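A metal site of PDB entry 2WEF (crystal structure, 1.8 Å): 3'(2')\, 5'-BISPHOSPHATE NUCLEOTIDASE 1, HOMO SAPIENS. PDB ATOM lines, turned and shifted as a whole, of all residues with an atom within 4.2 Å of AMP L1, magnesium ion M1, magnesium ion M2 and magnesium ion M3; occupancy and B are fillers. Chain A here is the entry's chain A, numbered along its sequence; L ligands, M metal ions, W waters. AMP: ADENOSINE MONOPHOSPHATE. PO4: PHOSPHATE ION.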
ATOM      1  N   LYS A  36     -28.691  20.064  15.862  1.00  0.00           N
ATOM      2  CA  LYS A  36     -29.082  18.667  15.625  1.00  0.00           C
ATOM      3  C   LYS A  36     -30.438  18.487  16.320  1.00  0.00           C
ATOM      4  O   LYS A  36     -31.443  18.915  15.751  1.00  0.00           O
ATOM      5  CB  LYS A  36     -28.016  17.698  16.044  1.00  0.00           C
ATOM      6  CG  LYS A  36     -26.822  17.824  15.035  1.00  0.00           C
ATOM      7  CD  LYS A  36     -25.729  16.765  15.145  1.00  0.00           C
ATOM      8  CE  LYS A  36     -25.135  16.653  16.510  1.00  0.00           C
ATOM      9  NZ  LYS A  36     -24.348  15.404  16.589  1.00  0.00           N
ATOM     10  N   ASP A  41     -27.530  21.089  21.221  1.00  0.00           N
ATOM     11  CA  ASP A  41     -26.988  19.858  20.576  1.00  0.00           C
ATOM     12  C   ASP A  41     -26.497  20.323  19.197  1.00  0.00           C
ATOM     13  O   ASP A  41     -27.248  20.252  18.183  1.00  0.00           O
ATOM     14  CB  ASP A  41     -28.097  18.771  20.500  1.00  0.00           C
ATOM     15  CG  ASP A  41     -27.677  17.454  19.805  1.00  0.00           C
ATOM     16  OD1 ASP A  41     -26.453  17.131  19.794  1.00  0.00           O
ATOM     17  OD2 ASP A  41     -28.579  16.747  19.225  1.00  0.00           O
ATOM     18  N   ASP A  47     -16.360  20.282  13.993  1.00  0.00           N
ATOM     19  CA  ASP A  47     -16.786  18.903  14.262  1.00  0.00           C
ATOM     20  C   ASP A  47     -16.680  18.077  13.024  1.00  0.00           C
ATOM     21  O   ASP A  47     -16.143  16.975  13.019  1.00  0.00           O
ATOM     22  CB  ASP A  47     -18.165  18.774  14.827  1.00  0.00           C
ATOM     23  CG  ASP A  47     -18.387  19.595  16.129  1.00  0.00           C
ATOM     24  OD1 ASP A  47     -18.583  20.819  16.013  1.00  0.00           O
ATOM     25  OD2 ASP A  47     -18.383  19.043  17.249  1.00  0.00           O
ATOM     26  N   GLU A  70     -18.775  10.322  16.557  1.00  0.00           N
ATOM     27  CA  GLU A  70     -20.039  10.914  16.973  1.00  0.00           C
ATOM     28  C   GLU A  70     -20.975  11.371  15.851  1.00  0.00           C
ATOM     29  O   GLU A  70     -22.208  11.090  15.872  1.00  0.00           O
ATOM     30  CB  GLU A  70     -19.762  12.129  17.825  1.00  0.00           C
ATOM     31  CG  GLU A  70     -20.999  12.810  18.314  1.00  0.00           C
ATOM     32  CD  GLU A  70     -20.783  14.036  19.129  1.00  0.00           C
ATOM     33  OE1 GLU A  70     -19.642  14.440  19.344  1.00  0.00           O
ATOM     34  OE2 GLU A  70     -21.791  14.545  19.639  1.00  0.00           O
ATOM     35  N   GLU A  71     -20.407  12.075  14.885  1.00  0.00           N
ATOM     36  CA  GLU A  71     -21.176  12.779  13.880  1.00  0.00           C
ATOM     37  C   GLU A  71     -21.610  11.802  12.775  1.00  0.00           C
ATOM     38  O   GLU A  71     -20.867  10.913  12.366  1.00  0.00           O
ATOM     39  CB  GLU A  71     -20.403  13.950  13.321  1.00  0.00           C
ATOM     40  CG  GLU A  71     -19.921  14.943  14.411  1.00  0.00           C
ATOM     41  CD  GLU A  71     -20.983  15.538  15.345  1.00  0.00           C
ATOM     42  OE1 GLU A  71     -22.189  15.754  14.937  1.00  0.00           O
ATOM     43  OE2 GLU A  71     -20.609  15.852  16.503  1.00  0.00           O
ATOM     44  N   ASP A 113     -14.665  11.253  19.429  1.00  0.00           N
ATOM     45  CA  ASP A 113     -15.369  12.471  19.583  1.00  0.00           C
ATOM     46  C   ASP A 113     -14.499  13.527  19.014  1.00  0.00           C
ATOM     47  O   ASP A 113     -13.507  13.890  19.609  1.00  0.00           O
ATOM     48  CB  ASP A 113     -15.714  12.759  21.047  1.00  0.00           C
ATOM     49  CG  ASP A 113     -16.743  13.879  21.170  1.00  0.00           C
ATOM     50  OD1 ASP A 113     -16.885  14.687  20.249  1.00  0.00           O
ATOM     51  OD2 ASP A 113     -17.359  13.913  22.229  1.00  0.00           O
ATOM     52  N   LEU A 115     -14.825  16.591  18.439  1.00  0.00           N
ATOM     53  CA  LEU A 115     -14.821  17.874  19.170  1.00  0.00           C
ATOM     54  C   LEU A 115     -15.829  17.670  20.276  1.00  0.00           C
ATOM     55  O   LEU A 115     -17.023  17.534  20.008  1.00  0.00           O
ATOM     56  CB  LEU A 115     -15.205  19.060  18.247  1.00  0.00           C
ATOM     57  CG  LEU A 115     -14.854  20.422  18.737  1.00  0.00           C
ATOM     58  CD1 LEU A 115     -15.150  21.491  17.624  1.00  0.00           C
ATOM     59  CD2 LEU A 115     -15.619  20.754  20.052  1.00  0.00           C
ATOM     60  N   ASP A 116     -15.348  17.646  21.504  1.00  0.00           N
ATOM     61  CA  ASP A 116     -16.152  17.509  22.706  1.00  0.00           C
ATOM     62  C   ASP A 116     -16.211  18.815  23.393  1.00  0.00           C
ATOM     63  O   ASP A 116     -15.170  19.432  23.674  1.00  0.00           O
ATOM     64  CB  ASP A 116     -15.632  16.396  23.663  1.00  0.00           C
ATOM     65  CG  ASP A 116     -16.537  16.206  24.858  1.00  0.00           C
ATOM     66  OD1 ASP A 116     -17.714  15.840  24.604  1.00  0.00           O
ATOM     67  OD2 ASP A 116     -16.033  16.385  26.020  1.00  0.00           O
ATOM     68  N   THR A 118     -18.758  21.118  22.085  1.00  0.00           N
ATOM     69  CA  THR A 118     -19.141  21.966  20.958  1.00  0.00           C
ATOM     70  C   THR A 118     -20.008  23.213  21.346  1.00  0.00           C
ATOM     71  O   THR A 118     -19.813  24.347  20.823  1.00  0.00           O
ATOM     72  CB  THR A 118     -19.861  21.119  19.912  1.00  0.00           C
ATOM     73  OG1 THR A 118     -19.093  20.009  19.499  1.00  0.00           O
ATOM     74  CG2 THR A 118     -20.284  21.985  18.707  1.00  0.00           C
ATOM     75  N   THR A 191     -22.213  19.302  34.150  1.00  0.00           N
ATOM     76  CA  THR A 191     -22.604  19.978  32.920  1.00  0.00           C
ATOM     77  C   THR A 191     -22.957  21.458  33.141  1.00  0.00           C
ATOM     78  O   THR A 191     -23.469  21.833  34.193  1.00  0.00           O
ATOM     79  CB  THR A 191     -23.835  19.238  32.311  1.00  0.00           C
ATOM     80  OG1 THR A 191     -24.263  19.890  31.093  1.00  0.00           O
ATOM     81  CG2 THR A 191     -24.994  19.184  33.355  1.00  0.00           C
ATOM     82  N   HIS A 194     -26.403  21.077  29.767  1.00  0.00           N
ATOM     83  CA  HIS A 194     -27.326  19.983  29.676  1.00  0.00           C
ATOM     84  C   HIS A 194     -27.829  19.577  31.066  1.00  0.00           C
ATOM     85  O   HIS A 194     -28.023  18.415  31.335  1.00  0.00           O
ATOM     86  CB  HIS A 194     -26.700  18.778  28.923  1.00  0.00           C
ATOM     87  CG  HIS A 194     -26.172  19.156  27.565  1.00  0.00           C
ATOM     88  ND1 HIS A 194     -24.822  19.249  27.264  1.00  0.00           N
ATOM     89  CD2 HIS A 194     -26.832  19.516  26.438  1.00  0.00           C
ATOM     90  CE1 HIS A 194     -24.691  19.682  26.016  1.00  0.00           C
ATOM     91  NE2 HIS A 194     -25.897  19.832  25.488  1.00  0.00           N
ATOM     92  N   VAL A 214     -19.008  23.435  33.776  1.00  0.00           N
ATOM     93  CA  VAL A 214     -18.146  23.525  32.620  1.00  0.00           C
ATOM     94  C   VAL A 214     -18.645  22.544  31.577  1.00  0.00           C
ATOM     95  O   VAL A 214     -19.310  21.522  31.880  1.00  0.00           O
ATOM     96  CB  VAL A 214     -16.664  23.236  32.957  1.00  0.00           C
ATOM     97  CG1 VAL A 214     -16.139  24.270  34.050  1.00  0.00           C
ATOM     98  CG2 VAL A 214     -16.473  21.782  33.436  1.00  0.00           C
ATOM     99  N   GLY A 215     -18.321  22.840  30.320  1.00  0.00           N
ATOM    100  CA  GLY A 215     -18.640  21.932  29.280  1.00  0.00           C
ATOM    101  C   GLY A 215     -17.561  20.842  29.072  1.00  0.00           C
ATOM    102  O   GLY A 215     -16.452  21.024  29.400  1.00  0.00           O
ATOM    103  N   GLY A 216     -17.980  19.742  28.475  1.00  0.00           N
ATOM    104  CA  GLY A 216     -17.114  18.676  28.002  1.00  0.00           C
ATOM    105  C   GLY A 216     -16.853  17.566  28.995  1.00  0.00           C
ATOM    106  O   GLY A 216     -16.546  17.798  30.188  1.00  0.00           O
ATOM    107  N   ALA A 217     -17.038  16.332  28.527  1.00  0.00           N
ATOM    108  CA  ALA A 217     -16.639  15.126  29.273  1.00  0.00           C
ATOM    109  C   ALA A 217     -15.090  15.025  29.399  1.00  0.00           C
ATOM    110  O   ALA A 217     -14.577  14.693  30.475  1.00  0.00           O
ATOM    111  CB  ALA A 217     -17.224  13.863  28.598  1.00  0.00           C
ATOM    112  N   LYS A 220     -13.868  17.580  31.947  1.00  0.00           N
ATOM    113  CA  LYS A 220     -14.157  17.266  33.367  1.00  0.00           C
ATOM    114  C   LYS A 220     -13.247  16.176  33.904  1.00  0.00           C
ATOM    115  O   LYS A 220     -12.917  16.212  35.048  1.00  0.00           O
ATOM    116  CB  LYS A 220     -15.652  17.005  33.589  1.00  0.00           C
ATOM    117  CG  LYS A 220     -16.458  18.327  33.568  1.00  0.00           C
ATOM    118  CD  LYS A 220     -17.975  18.244  33.885  1.00  0.00           C
ATOM    119  CE  LYS A 220     -18.832  17.777  32.785  1.00  0.00           C
ATOM    120  NZ  LYS A 220     -18.830  18.837  31.675  1.00  0.00           N
ATOM    121  N   PHE A 234     -22.813  13.287  36.788  1.00  0.00           N
ATOM    122  CA  PHE A 234     -23.766  13.614  35.716  1.00  0.00           C
ATOM    123  C   PHE A 234     -24.891  12.542  35.677  1.00  0.00           C
ATOM    124  O   PHE A 234     -24.793  11.535  35.001  1.00  0.00           O
ATOM    125  CB  PHE A 234     -23.016  13.654  34.384  1.00  0.00           C
ATOM    126  CG  PHE A 234     -23.877  14.049  33.240  1.00  0.00           C
ATOM    127  CD1 PHE A 234     -24.572  15.260  33.295  1.00  0.00           C
ATOM    128  CD2 PHE A 234     -23.942  13.273  32.116  1.00  0.00           C
ATOM    129  CE1 PHE A 234     -25.376  15.674  32.167  1.00  0.00           C
ATOM    130  CE2 PHE A 234     -24.724  13.623  31.029  1.00  0.00           C
ATOM    131  CZ  PHE A 234     -25.459  14.835  31.054  1.00  0.00           C
ATOM    132  N   GLY A 238     -27.290  11.205  27.898  1.00  0.00           N
ATOM    133  CA  GLY A 238     -26.813  12.344  27.119  1.00  0.00           C
ATOM    134  C   GLY A 238     -25.435  12.171  26.606  1.00  0.00           C
ATOM    135  O   GLY A 238     -25.124  12.536  25.480  1.00  0.00           O
ATOM    136  N   CYS A 239     -24.583  11.613  27.439  1.00  0.00           N
ATOM    137  CA  CYS A 239     -23.279  11.389  26.962  1.00  0.00           C
ATOM    138  C   CYS A 239     -23.172   9.959  26.411  1.00  0.00           C
ATOM    139  O   CYS A 239     -24.022   9.140  26.693  1.00  0.00           O
ATOM    140  CB  CYS A 239     -22.263  11.775  27.936  1.00  0.00           C
ATOM    141  SG  CYS A 239     -21.871  10.612  29.132  1.00  0.00           S
ATOM    142  N   ASP A 243     -17.592   9.945  24.453  1.00  0.00           N
ATOM    143  CA  ASP A 243     -17.346  10.958  25.489  1.00  0.00           C
ATOM    144  C   ASP A 243     -16.546  10.366  26.628  1.00  0.00           C
ATOM    145  O   ASP A 243     -15.774  11.070  27.314  1.00  0.00           O
ATOM    146  CB  ASP A 243     -18.724  11.460  26.054  1.00  0.00           C
ATOM    147  CG  ASP A 243     -19.470  12.293  25.064  1.00  0.00           C
ATOM    148  OD1 ASP A 243     -18.903  13.312  24.708  1.00  0.00           O
ATOM    149  OD2 ASP A 243     -20.593  11.916  24.635  1.00  0.00           O
HETATM  150  P   AMP L   1     -21.579  18.328  29.044  1.00  0.00           P
HETATM  151  O1P AMP L   1     -21.091  18.068  30.453  1.00  0.00           O
HETATM  152  O2P AMP L   1     -22.953  18.874  29.062  1.00  0.00           O
HETATM  153  O3P AMP L   1     -20.656  19.036  28.117  1.00  0.00           O
HETATM  154  O5' AMP L   1     -21.833  16.882  28.427  1.00  0.00           O
HETATM  155  C5' AMP L   1     -20.756  15.971  28.145  1.00  0.00           C
HETATM  156  C4' AMP L   1     -20.860  15.420  26.730  1.00  0.00           C
HETATM  157  O4' AMP L   1     -22.075  14.729  26.542  1.00  0.00           O
HETATM  158  C3' AMP L   1     -20.929  16.485  25.591  1.00  0.00           C
HETATM  159  O3' AMP L   1     -20.698  15.867  24.277  1.00  0.00           O
HETATM  160  C2' AMP L   1     -22.350  16.816  25.450  1.00  0.00           C
HETATM  161  O2' AMP L   1     -22.634  17.428  24.195  1.00  0.00           O
HETATM  162  C1' AMP L   1     -22.905  15.406  25.603  1.00  0.00           C
HETATM  163  N9  AMP L   1     -24.226  15.587  26.160  1.00  0.00           N
HETATM  164  C8  AMP L   1     -24.566  15.555  27.458  1.00  0.00           C
HETATM  165  N7  AMP L   1     -25.879  15.721  27.606  1.00  0.00           N
HETATM  166  C5  AMP L   1     -26.377  15.932  26.360  1.00  0.00           C
HETATM  167  C6  AMP L   1     -27.698  16.204  25.782  1.00  0.00           C
HETATM  168  N6  AMP L   1     -28.775  16.329  26.560  1.00  0.00           N
HETATM  169  N1  AMP L   1     -27.773  16.333  24.428  1.00  0.00           N
HETATM  170  C2  AMP L   1     -26.706  16.213  23.630  1.00  0.00           C
HETATM  171  N3  AMP L   1     -25.473  15.953  24.086  1.00  0.00           N
HETATM  172  C4  AMP L   1     -25.289  15.802  25.420  1.00  0.00           C
HETATM  173  P   PO4 L   2     -20.135  17.257  21.601  1.00  0.00           P
HETATM  174  O1  PO4 L   2     -21.584  16.759  21.728  1.00  0.00           O
HETATM  175  O2  PO4 L   2     -19.915  18.489  22.492  1.00  0.00           O
HETATM  176  O3  PO4 L   2     -19.113  16.107  21.861  1.00  0.00           O
HETATM  177  O4  PO4 L   2     -19.939  17.614  20.060  1.00  0.00           O
HETATM  178 MG    MG M   1     -18.908  14.788  23.311  1.00  0.00          MG
HETATM  179 MG    MG M   2     -18.426  16.008  19.876  1.00  0.00          MG
HETATM  180 MG    MG M   3     -22.882  16.077  20.365  1.00  0.00          MG
HETATM  181  O   HOH W   1     -21.628  15.912  31.668  1.00  0.00           O
HETATM  182  O   HOH W   2     -25.634  13.031  22.977  1.00  0.00           O
HETATM  183  O   HOH W   3     -22.135  21.728  29.238  1.00  0.00           O
HETATM  184  O   HOH W   4     -20.629  13.575  22.465  1.00  0.00           O
HETATM  185  O   HOH W   5     -28.651  15.796  29.956  1.00  0.00           O
HETATM  186  O   HOH W   6     -18.281  16.413  17.832  1.00  0.00           O
HETATM  187  O   HOH W   7     -24.554  15.291  19.448  1.00  0.00           O
HETATM  188  O   HOH W   8     -24.247  17.488  20.977  1.00  0.00           O
HETATM  189  O   HOH W   9     -22.394  17.081  18.540  1.00  0.00           O
HETATM  190  O   HOH W  10     -21.477  20.566  26.165  1.00  0.00           O
HETATM  191  O   HOH W  11     -21.651  20.310  23.423  1.00  0.00           O
HETATM  192  O   HOH W  12     -23.501  14.805  22.065  1.00  0.00           O
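O2P of AMP L1 is in hydrogen-bond range of ND1 of His 194 (2.6 Å). The side-chain hydroxyl (OG1) of Thr 191 is in hydrogen-bond range of an oxygen (O2P) of AMP L1, at 2.6 Å. An oxygen (O1P) of AMP L1 is in salt-bridge range of the side-chain amino group (NZ) of Lys 220 (2.7 Å). The backbone NH of Gly 216 sits at hydrogen-bond distance from an oxygen (O3P) of AMP L1 (2.8 Å).
Three residues have an atom within 4 Å of magnesium ion M1: Asp 113, Asp 116 and Asp 243. Along chain A the residues within 4 Å of magnesium ion M1 span positions 113 to 243.
OE1 of Glu 70 binds magnesium ion M2, at 2.1 Å. Magnesium ion M2 is bound by the side-chain carboxylate (OD1) of Asp 113, 2.1 Å away. The backbone carbonyl oxygen (O) of Leu 115 binds magnesium ion M2 (2.1 Å). Magnesium ion M2 is bound by water W6. Magnesium ion M2 is bound by an oxygen (O3) of PO4 L2 (2.1 Å). O4 of PO4 L2 binds magnesium ion M2 (2.2 Å). Magnesium ion M2 has six donor atoms within binding distance.
OD1 of Asp 41 touches magnesium ion M3 (3.8 Å). Two residues have an atom within 4 Å of magnesium ion M3: Asp 41 and Glu 70.
OD2 of Asp 116 lies within hydrogen-bond range of N of Ala 217. The side-chain hydroxyl of Thr 118 lies close to the backbone carbonyl oxygen of Leu 115 (3.3 Å). The side-chain hydroxyl of Thr 191 sits at hydrogen-bond distance from the backbone NH of His 194 (2.8 Å). The backbone carbonyl oxygen (O) of Gly 216 sits at hydrogen-bond distance from the side-chain amino group (NZ) of Lys 220 (2.9 Å). The backbone carbonyl oxygen (O) of Val 214 lies within hydrogen-bond range of the side-chain amino group (NZ) of Lys 220 (2.7 Å). The backbone NH of Lys 36 is in hydrogen-bond range of the backbone carbonyl oxygen of Asp 41 (2.7 Å).
O3 of PO4 L2 is bound to magnesium ion M1, at 2.0 Å. OD1 of Asp 243 is bound to magnesium ion M1 (2.0 Å). OD1 of Asp 116 is bound to magnesium ion M1 (2.1 Å). OD2 of Asp 113 is bound to magnesium ion M1, at 2.1 Å. Water W4 binds magnesium ion M1, 2.3 Å away. Magnesium ion M1 is bound by an oxygen (O3') of AMP L1, at 2.3 Å. Magnesium ion M1 has six donor atoms within binding distance.
The backbone carbonyl oxygen (O) of Gly 238 lies close to a nitrogen (N9) of AMP L1 (3.3 Å). Residues that only touch AMP L1: Cys 239 (3.3 Å), Phe 234 (3.6 Å), Gly 215 (3.7 Å), Ala 217 (3.8 Å) and Asp 41 (3.95 Å). 12 residues have an atom within 4 Å of AMP L1: Asp 41, Asp 116, Thr 191, His 194, Gly 215, Gly 216, Ala 217, Lys 220, Phe 234, Gly 238, Cys 239 and Asp 243.
Water W6 lies within hydrogen-bond range of OD2 of Asp 47 (2.7 Å) and OE2 of Glu 71 (2.7 Å). Water W9 lies within hydrogen-bond range of OE2 of Glu 71 and NZ of Lys 36. Water W7 lies within hydrogen-bond range of the side-chain carboxylate of Asp 41 (2.7 Å) and the side-chain amino group of Lys 36 (2.9 Å). Water W2 bridges O of Gly 238 and N3 of AMP L1. Water W11 lies within hydrogen-bond range of O2' of AMP L1 (3.1 Å) and N of Thr 118 (3.3 Å). Water W5 lies within hydrogen-bond range of the backbone carbonyl oxygen of His 194 (3.0 Å) and a nitrogen (N6) of AMP L1 (3.4 Å).
Magnesium ion M3 is bound by an oxygen (O1) of PO4 L2, the side-chain carboxylate of Glu 70, water W8, water W7, water W9 and water W12.
Four residues have an atom within 4 Å of magnesium ion M2: Glu 70, Asp 113, Leu 115 and Asp 116. The nearest printed residue that does not touch magnesium ion M2 is Asp 47 (4.01 Å).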
